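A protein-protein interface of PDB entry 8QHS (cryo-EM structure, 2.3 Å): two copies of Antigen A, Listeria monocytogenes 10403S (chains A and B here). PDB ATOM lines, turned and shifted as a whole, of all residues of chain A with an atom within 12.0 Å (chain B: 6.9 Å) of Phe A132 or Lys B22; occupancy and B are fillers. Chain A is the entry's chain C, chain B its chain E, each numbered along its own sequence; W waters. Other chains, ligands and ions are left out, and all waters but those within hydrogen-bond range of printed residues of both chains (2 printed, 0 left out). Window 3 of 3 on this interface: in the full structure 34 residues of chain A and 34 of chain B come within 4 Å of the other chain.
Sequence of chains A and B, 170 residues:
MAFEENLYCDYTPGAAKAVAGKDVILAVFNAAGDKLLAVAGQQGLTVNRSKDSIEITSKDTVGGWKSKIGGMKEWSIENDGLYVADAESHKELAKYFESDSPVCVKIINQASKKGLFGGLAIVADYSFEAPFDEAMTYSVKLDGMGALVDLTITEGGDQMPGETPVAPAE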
ATOM      1  N   LEU A  82     -31.569  13.652   7.734  1.00  0.00           N
ATOM      2  CA  LEU A  82     -31.546  13.962   9.156  1.00  0.00           C
ATOM      3  C   LEU A  82     -31.664  12.689   9.978  1.00  0.00           C
ATOM      4  O   LEU A  82     -32.574  11.886   9.780  1.00  0.00           O
ATOM      5  CB  LEU A  82     -32.678  14.918   9.508  1.00  0.00           C
ATOM      6  CG  LEU A  82     -32.707  16.188   8.670  1.00  0.00           C
ATOM      7  CD1 LEU A  82     -34.036  16.876   8.804  1.00  0.00           C
ATOM      8  CD2 LEU A  82     -31.588  17.106   9.076  1.00  0.00           C
ATOM      9  N   TYR A  83     -30.739  12.510  10.908  1.00  0.00           N
ATOM     10  CA  TYR A  83     -30.659  11.303  11.712  1.00  0.00           C
ATOM     11  C   TYR A  83     -31.438  11.473  13.006  1.00  0.00           C
ATOM     12  O   TYR A  83     -31.181  12.402  13.773  1.00  0.00           O
ATOM     13  CB  TYR A  83     -29.210  10.948  12.034  1.00  0.00           C
ATOM     14  CG  TYR A  83     -29.094   9.672  12.822  1.00  0.00           C
ATOM     15  CD1 TYR A  83     -29.689   8.503  12.372  1.00  0.00           C
ATOM     16  CD2 TYR A  83     -28.410   9.635  14.024  1.00  0.00           C
ATOM     17  CE1 TYR A  83     -29.592   7.343  13.082  1.00  0.00           C
ATOM     18  CE2 TYR A  83     -28.305   8.474  14.744  1.00  0.00           C
ATOM     19  CZ  TYR A  83     -28.897   7.329  14.269  1.00  0.00           C
ATOM     20  OH  TYR A  83     -28.795   6.166  14.983  1.00  0.00           O
ATOM     21  N   PHE A 128     -22.458   8.990  10.401  1.00  0.00           N
ATOM     22  CA  PHE A 128     -23.167  10.109  11.000  1.00  0.00           C
ATOM     23  C   PHE A 128     -22.253  11.317  11.125  1.00  0.00           C
ATOM     24  O   PHE A 128     -21.048  11.178  11.334  1.00  0.00           O
ATOM     25  CB  PHE A 128     -23.723   9.723  12.374  1.00  0.00           C
ATOM     26  CG  PHE A 128     -24.446   8.417  12.371  1.00  0.00           C
ATOM     27  CD1 PHE A 128     -25.764   8.344  11.979  1.00  0.00           C
ATOM     28  CD2 PHE A 128     -23.792   7.251  12.718  1.00  0.00           C
ATOM     29  CE1 PHE A 128     -26.419   7.140  11.950  1.00  0.00           C
ATOM     30  CE2 PHE A 128     -24.444   6.052  12.689  1.00  0.00           C
ATOM     31  CZ  PHE A 128     -25.764   5.996  12.309  1.00  0.00           C
ATOM     32  N   GLU A 129     -22.838  12.498  10.986  1.00  0.00           N
ATOM     33  CA  GLU A 129     -22.146  13.759  11.197  1.00  0.00           C
ATOM     34  C   GLU A 129     -22.968  14.633  12.125  1.00  0.00           C
ATOM     35  O   GLU A 129     -24.192  14.704  11.997  1.00  0.00           O
ATOM     36  CB  GLU A 129     -21.887  14.485   9.880  1.00  0.00           C
ATOM     37  CG  GLU A 129     -20.503  14.244   9.338  1.00  0.00           C
ATOM     38  CD  GLU A 129     -20.493  13.800   7.901  1.00  0.00           C
ATOM     39  OE1 GLU A 129     -19.546  13.086   7.510  1.00  0.00           O
ATOM     40  OE2 GLU A 129     -21.420  14.176   7.155  1.00  0.00           O
ATOM     41  N   ALA A 130     -22.292  15.298  13.057  1.00  0.00           N
ATOM     42  CA  ALA A 130     -22.934  16.183  14.026  1.00  0.00           C
ATOM     43  C   ALA A 130     -22.136  17.476  14.120  1.00  0.00           C
ATOM     44  O   ALA A 130     -21.291  17.636  15.006  1.00  0.00           O
ATOM     45  CB  ALA A 130     -23.064  15.504  15.388  1.00  0.00           C
ATOM     46  N   PRO A 131     -22.369  18.416  13.211  1.00  0.00           N
ATOM     47  CA  PRO A 131     -21.752  19.737  13.355  1.00  0.00           C
ATOM     48  C   PRO A 131     -22.460  20.536  14.436  1.00  0.00           C
ATOM     49  O   PRO A 131     -23.659  20.378  14.659  1.00  0.00           O
ATOM     50  CB  PRO A 131     -21.936  20.373  11.971  1.00  0.00           C
ATOM     51  CG  PRO A 131     -22.482  19.289  11.093  1.00  0.00           C
ATOM     52  CD  PRO A 131     -23.164  18.321  11.980  1.00  0.00           C
ATOM     53  N   PHE A 132     -21.707  21.402  15.110  1.00  0.00           N
ATOM     54  CA  PHE A 132     -22.268  22.115  16.251  1.00  0.00           C
ATOM     55  C   PHE A 132     -23.323  23.124  15.817  1.00  0.00           C
ATOM     56  O   PHE A 132     -24.177  23.515  16.615  1.00  0.00           O
ATOM     57  CB  PHE A 132     -21.154  22.801  17.046  1.00  0.00           C
ATOM     58  CG  PHE A 132     -20.717  24.111  16.475  1.00  0.00           C
ATOM     59  CD1 PHE A 132     -21.206  25.300  16.981  1.00  0.00           C
ATOM     60  CD2 PHE A 132     -19.818  24.156  15.428  1.00  0.00           C
ATOM     61  CE1 PHE A 132     -20.813  26.496  16.450  1.00  0.00           C
ATOM     62  CE2 PHE A 132     -19.417  25.351  14.900  1.00  0.00           C
ATOM     63  CZ  PHE A 132     -19.915  26.524  15.412  1.00  0.00           C
ATOM     64  N   ASP A 133     -23.290  23.551  14.562  1.00  0.00           N
ATOM     65  CA  ASP A 133     -24.192  24.590  14.094  1.00  0.00           C
ATOM     66  C   ASP A 133     -25.287  24.073  13.167  1.00  0.00           C
ATOM     67  O   ASP A 133     -26.043  24.878  12.621  1.00  0.00           O
ATOM     68  CB  ASP A 133     -23.395  25.694  13.394  1.00  0.00           C
ATOM     69  CG  ASP A 133     -22.502  25.164  12.293  1.00  0.00           C
ATOM     70  OD1 ASP A 133     -22.079  23.993  12.364  1.00  0.00           O
ATOM     71  OD2 ASP A 133     -22.218  25.926  11.350  1.00  0.00           O
ATOM     72  N   GLU A 134     -25.402  22.763  12.987  1.00  0.00           N
ATOM     73  CA  GLU A 134     -26.390  22.179  12.094  1.00  0.00           C
ATOM     74  C   GLU A 134     -27.110  21.038  12.793  1.00  0.00           C
ATOM     75  O   GLU A 134     -26.968  20.831  13.997  1.00  0.00           O
ATOM     76  CB  GLU A 134     -25.739  21.675  10.802  1.00  0.00           C
ATOM     77  CG  GLU A 134     -25.112  22.767   9.969  1.00  0.00           C
ATOM     78  CD  GLU A 134     -24.078  22.243   9.001  1.00  0.00           C
ATOM     79  OE1 GLU A 134     -24.369  21.257   8.294  1.00  0.00           O
ATOM     80  OE2 GLU A 134     -22.972  22.815   8.946  1.00  0.00           O
ATOM     81  N   ALA A 135     -27.898  20.303  12.021  1.00  0.00           N
ATOM     82  CA  ALA A 135     -28.562  19.122  12.547  1.00  0.00           C
ATOM     83  C   ALA A 135     -27.707  17.885  12.315  1.00  0.00           C
ATOM     84  O   ALA A 135     -26.921  17.816  11.371  1.00  0.00           O
ATOM     85  CB  ALA A 135     -29.929  18.946  11.897  1.00  0.00           C
ATOM     86  N   MET A 136     -27.858  16.907  13.199  1.00  0.00           N
ATOM     87  CA  MET A 136     -27.158  15.644  13.027  1.00  0.00           C
ATOM     88  C   MET A 136     -27.707  14.898  11.817  1.00  0.00           C
ATOM     89  O   MET A 136     -28.916  14.732  11.663  1.00  0.00           O
ATOM     90  CB  MET A 136     -27.293  14.792  14.285  1.00  0.00           C
ATOM     91  CG  MET A 136     -26.575  13.465  14.219  1.00  0.00           C
ATOM     92  SD  MET A 136     -26.787  12.491  15.706  1.00  0.00           S
ATOM     93  CE  MET A 136     -25.561  11.226  15.447  1.00  0.00           C
ATOM     94  N   THR A 137     -26.810  14.455  10.945  1.00  0.00           N
ATOM     95  CA  THR A 137     -27.207  13.758   9.736  1.00  0.00           C
ATOM     96  C   THR A 137     -26.655  12.345   9.748  1.00  0.00           C
ATOM     97  O   THR A 137     -25.697  12.029  10.450  1.00  0.00           O
ATOM     98  CB  THR A 137     -26.744  14.482   8.460  1.00  0.00           C
ATOM     99  OG1 THR A 137     -25.344  14.766   8.536  1.00  0.00           O
ATOM    100  CG2 THR A 137     -27.514  15.769   8.261  1.00  0.00           C
ATOM    101  N   VAL B  19     -32.333  16.122  15.357  1.00  0.00           N
ATOM    102  CA  VAL B  19     -31.465  16.353  16.501  1.00  0.00           C
ATOM    103  C   VAL B  19     -30.445  17.408  16.111  1.00  0.00           C
ATOM    104  O   VAL B  19     -29.775  17.279  15.082  1.00  0.00           O
ATOM    105  CB  VAL B  19     -30.769  15.057  16.955  1.00  0.00           C
ATOM    106  CG1 VAL B  19     -29.904  15.316  18.168  1.00  0.00           C
ATOM    107  CG2 VAL B  19     -31.795  13.980  17.240  1.00  0.00           C
ATOM    108  N   ALA B  20     -30.341  18.458  16.920  1.00  0.00           N
ATOM    109  CA  ALA B  20     -29.291  19.444  16.712  1.00  0.00           C
ATOM    110  C   ALA B  20     -27.928  18.807  16.931  1.00  0.00           C
ATOM    111  O   ALA B  20     -27.720  18.066  17.894  1.00  0.00           O
ATOM    112  CB  ALA B  20     -29.477  20.634  17.649  1.00  0.00           C
ATOM    113  N   GLY B  21     -26.997  19.092  16.021  1.00  0.00           N
ATOM    114  CA  GLY B  21     -25.675  18.498  16.117  1.00  0.00           C
ATOM    115  C   GLY B  21     -24.946  18.873  17.394  1.00  0.00           C
ATOM    116  O   GLY B  21     -24.099  18.123  17.874  1.00  0.00           O
ATOM    117  N   LYS B  22     -25.282  20.027  17.971  1.00  0.00           N
ATOM    118  CA  LYS B  22     -24.586  20.498  19.164  1.00  0.00           C
ATOM    119  C   LYS B  22     -24.911  19.643  20.383  1.00  0.00           C
ATOM    120  O   LYS B  22     -24.203  19.703  21.392  1.00  0.00           O
ATOM    121  CB  LYS B  22     -24.933  21.958  19.433  1.00  0.00           C
ATOM    122  CG  LYS B  22     -26.344  22.182  19.901  1.00  0.00           C
ATOM    123  CD  LYS B  22     -26.632  23.653  20.060  1.00  0.00           C
ATOM    124  CE  LYS B  22     -28.090  23.895  20.381  1.00  0.00           C
ATOM    125  NZ  LYS B  22     -28.472  23.309  21.688  1.00  0.00           N
ATOM    126  N   ASP B  23     -25.976  18.845  20.317  1.00  0.00           N
ATOM    127  CA  ASP B  23     -26.325  18.005  21.455  1.00  0.00           C
ATOM    128  C   ASP B  23     -25.611  16.665  21.395  1.00  0.00           C
ATOM    129  O   ASP B  23     -25.629  15.901  22.364  1.00  0.00           O
ATOM    130  CB  ASP B  23     -27.837  17.809  21.528  1.00  0.00           C
ATOM    131  CG  ASP B  23     -28.582  19.117  21.670  1.00  0.00           C
ATOM    132  OD1 ASP B  23     -28.614  19.669  22.787  1.00  0.00           O
ATOM    133  OD2 ASP B  23     -29.163  19.581  20.672  1.00  0.00           O
ATOM    134  N   VAL B  24     -24.969  16.365  20.271  1.00  0.00           N
ATOM    135  CA  VAL B  24     -24.257  15.104  20.127  1.00  0.00           C
ATOM    136  C   VAL B  24     -22.767  15.351  20.284  1.00  0.00           C
ATOM    137  O   VAL B  24     -22.137  16.001  19.443  1.00  0.00           O
ATOM    138  CB  VAL B  24     -24.587  14.459  18.774  1.00  0.00           C
ATOM    139  CG1 VAL B  24     -23.881  13.133  18.627  1.00  0.00           C
ATOM    140  CG2 VAL B  24     -26.085  14.295  18.635  1.00  0.00           C
ATOM    141  N   ILE B  25     -22.189  14.828  21.362  1.00  0.00           N
ATOM    142  CA  ILE B  25     -20.807  15.126  21.707  1.00  0.00           C
ATOM    143  C   ILE B  25     -20.022  13.836  21.885  1.00  0.00           C
ATOM    144  O   ILE B  25     -20.572  12.775  22.181  1.00  0.00           O
ATOM    145  CB  ILE B  25     -20.691  15.998  22.979  1.00  0.00           C
ATOM    146  CG1 ILE B  25     -21.241  15.255  24.185  1.00  0.00           C
ATOM    147  CG2 ILE B  25     -21.410  17.325  22.798  1.00  0.00           C
ATOM    148  CD1 ILE B  25     -20.240  15.056  25.263  1.00  0.00           C
ATOM    149  N   GLN B  42     -15.176  20.996  21.422  1.00  0.00           N
ATOM    150  CA  GLN B  42     -15.465  20.261  20.198  1.00  0.00           C
ATOM    151  C   GLN B  42     -16.549  20.955  19.382  1.00  0.00           C
ATOM    152  O   GLN B  42     -17.492  21.528  19.930  1.00  0.00           O
ATOM    153  CB  GLN B  42     -15.871  18.825  20.522  1.00  0.00           C
ATOM    154  CG  GLN B  42     -17.137  18.663  21.324  1.00  0.00           C
ATOM    155  CD  GLN B  42     -17.452  17.214  21.599  1.00  0.00           C
ATOM    156  OE1 GLN B  42     -17.963  16.510  20.737  1.00  0.00           O
ATOM    157  NE2 GLN B  42     -17.144  16.759  22.801  1.00  0.00           N
ATOM    158  N   GLN B  43     -16.394  20.917  18.068  1.00  0.00           N
ATOM    159  CA  GLN B  43     -17.304  21.570  17.144  1.00  0.00           C
ATOM    160  C   GLN B  43     -17.840  20.647  16.066  1.00  0.00           C
ATOM    161  O   GLN B  43     -18.997  20.781  15.683  1.00  0.00           O
ATOM    162  CB  GLN B  43     -16.619  22.773  16.480  1.00  0.00           C
ATOM    163  CG  GLN B  43     -16.212  23.852  17.461  1.00  0.00           C
ATOM    164  CD  GLN B  43     -15.495  25.010  16.817  1.00  0.00           C
ATOM    165  OE1 GLN B  43     -15.937  26.147  16.899  1.00  0.00           O
ATOM    166  NE2 GLN B  43     -14.371  24.727  16.181  1.00  0.00           N
ATOM    167  N   GLY B  44     -17.040  19.714  15.578  1.00  0.00           N
ATOM    168  CA  GLY B  44     -17.496  18.796  14.562  1.00  0.00           C
ATOM    169  C   GLY B  44     -17.295  17.356  14.961  1.00  0.00           C
ATOM    170  O   GLY B  44     -16.316  17.018  15.623  1.00  0.00           O
ATOM    171  N   LEU B  45     -18.220  16.495  14.563  1.00  0.00           N
ATOM    172  CA  LEU B  45     -18.184  15.087  14.910  1.00  0.00           C
ATOM    173  C   LEU B  45     -18.567  14.260  13.695  1.00  0.00           C
ATOM    174  O   LEU B  45     -19.586  14.524  13.057  1.00  0.00           O
ATOM    175  CB  LEU B  45     -19.127  14.797  16.076  1.00  0.00           C
ATOM    176  CG  LEU B  45     -19.082  13.409  16.705  1.00  0.00           C
ATOM    177  CD1 LEU B  45     -17.687  13.083  17.189  1.00  0.00           C
ATOM    178  CD2 LEU B  45     -20.076  13.345  17.844  1.00  0.00           C
ATOM    179  N   ASN B 109     -25.983  11.810  23.163  1.00  0.00           N
ATOM    180  CA  ASN B 109     -26.890  12.935  22.995  1.00  0.00           C
ATOM    181  C   ASN B 109     -27.084  13.542  24.378  1.00  0.00           C
ATOM    182  O   ASN B 109     -27.768  12.959  25.221  1.00  0.00           O
ATOM    183  CB  ASN B 109     -28.213  12.478  22.389  1.00  0.00           C
ATOM    184  CG  ASN B 109     -29.111  13.629  21.978  1.00  0.00           C
ATOM    185  OD1 ASN B 109     -29.068  14.708  22.555  1.00  0.00           O
ATOM    186  ND2 ASN B 109     -29.944  13.393  20.981  1.00  0.00           N
ATOM    187  N   GLN B 110     -26.459  14.695  24.621  1.00  0.00           N
ATOM    188  CA  GLN B 110     -26.485  15.267  25.962  1.00  0.00           C
ATOM    189  C   GLN B 110     -27.842  15.883  26.276  1.00  0.00           C
ATOM    190  O   GLN B 110     -28.190  16.064  27.447  1.00  0.00           O
ATOM    191  CB  GLN B 110     -25.369  16.299  26.128  1.00  0.00           C
ATOM    192  CG  GLN B 110     -25.599  17.609  25.406  1.00  0.00           C
ATOM    193  CD  GLN B 110     -24.492  18.613  25.651  1.00  0.00           C
ATOM    194  OE1 GLN B 110     -23.573  18.751  24.848  1.00  0.00           O
ATOM    195  NE2 GLN B 110     -24.578  19.327  26.765  1.00  0.00           N
ATOM    196  N   ALA B 111     -28.621  16.215  25.247  1.00  0.00           N
ATOM    197  CA  ALA B 111     -29.947  16.773  25.482  1.00  0.00           C
ATOM    198  C   ALA B 111     -30.942  15.691  25.878  1.00  0.00           C
ATOM    199  O   ALA B 111     -31.739  15.877  26.803  1.00  0.00           O
ATOM    200  CB  ALA B 111     -30.434  17.516  24.241  1.00  0.00           C
HETATM  201  O   HOH W   1     -30.910  15.013  13.188  1.00  0.00           O
HETATM  202  O   HOH W   2     -26.624  22.455  16.222  1.00  0.00           O
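Water W1 lies within hydrogen-bond range of O of Met A136 (2.5 Å), O of Tyr A83 (2.7 Å) and N of Val B19 (2.8 Å). Water W2 lies within hydrogen-bond range of O of Phe A132, O of Glu A134, N of Lys B22 and N of Gly B21.
N of Ala A130 is in hydrogen-bond range of O of Leu B45, 2.8 Å away. O of Val B19 lies within hydrogen-bond range of N of Met A136 (2.7 Å). The backbone carbonyl oxygen (O) of Glu A134 is in hydrogen-bond range of the backbone NH (N) of Gly B21 (2.7 Å). N of Phe A132 is in hydrogen-bond range of O of Gln B43 (2.8 Å).
Leu B45 touches Glu A129. Gly B21 touches Ala A130. O of Ala A130 touches O of Gln B43, 3.95 Å away. Ala A130 touches Gly B44. Gly B21 touches Pro A131 (CA to O, 3.1 Å). Pro A131 touches Lys B22. Phe A132 touches Lys B22. Glu A134 touches Ala B20 (O to C, 3.7 Å). CA of Ala A135 touches O of Val B19, at 3.4 Å. N of Met A136 touches N of Gly B21 (3.7 Å).
Of the 12 printed residues of chain A, 8 touch a printed residue of chain B. Hydrophobic or aromatic side chains of chain A that line the printed part of chain B: Ala A130, Phe A132, Ala A135 and Met A136. Of the 14 printed residues of chain B, 8 touch a printed residue of chain A. Hydrophobic or aromatic side chains of chain B that line the printed part of chain A: Val B19, Val B24 and Leu B45. Among the printed residues, 19 pairs touch across the chains. Among the printed residues, no Asp or Glu carboxylate lies within 4 Å of a Lys or Arg side-chain nitrogen of the other chain.
Of the printed residues of chain B, Glu A129 touches Leu B45. Of the printed residues of chain B, Ala A130 touches Gly B21, Val B24, Gln B43, Gly B44 and Leu B45. Of the printed residues of chain B, Pro A131 touches Gly B21, Lys B22 and Gln B43. Of chain B, only Lys B22 (3.3 Å) and Gln B43 (2.8 Å) come within 4 Å of Phe A132. Printed residues of chain A within 4 Å of Ala B20: Glu A134 (3.7 Å). Gly B21 touches just these residues of chain A: Ala A130, Pro A131, Glu A134, Ala A135 and Met A136. Val B24 touches just these residues of chain A: Ala A130 and Met A136. No residue of chain A comes within 4 Å of Ile B25. Of chain A, only Ala A130 (3.95 Å), Pro A131 (3.7 Å) and Phe A132 (2.8 Å) come within 4 Å of Gln B43. Printed residues of chain A within 4 Å of Gly B44: Ala A130 (3.99 Å). Gln B110 touches none of the printed residues of chain A. The nearest residue of chain A that does not touch Lys B22 is Glu A134 (4.4 Å).
O of Glu A129 lies within hydrogen-bond range of N of Thr A137, at 2.8 Å. The side-chain amino group of Lys B22 is in salt-bridge range of the side-chain carboxylate of Asp B23 (3.8 Å). O of Met A136 lies within hydrogen-bond range of N of Tyr A83 (3.0 Å).
No position is printed for both chains.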
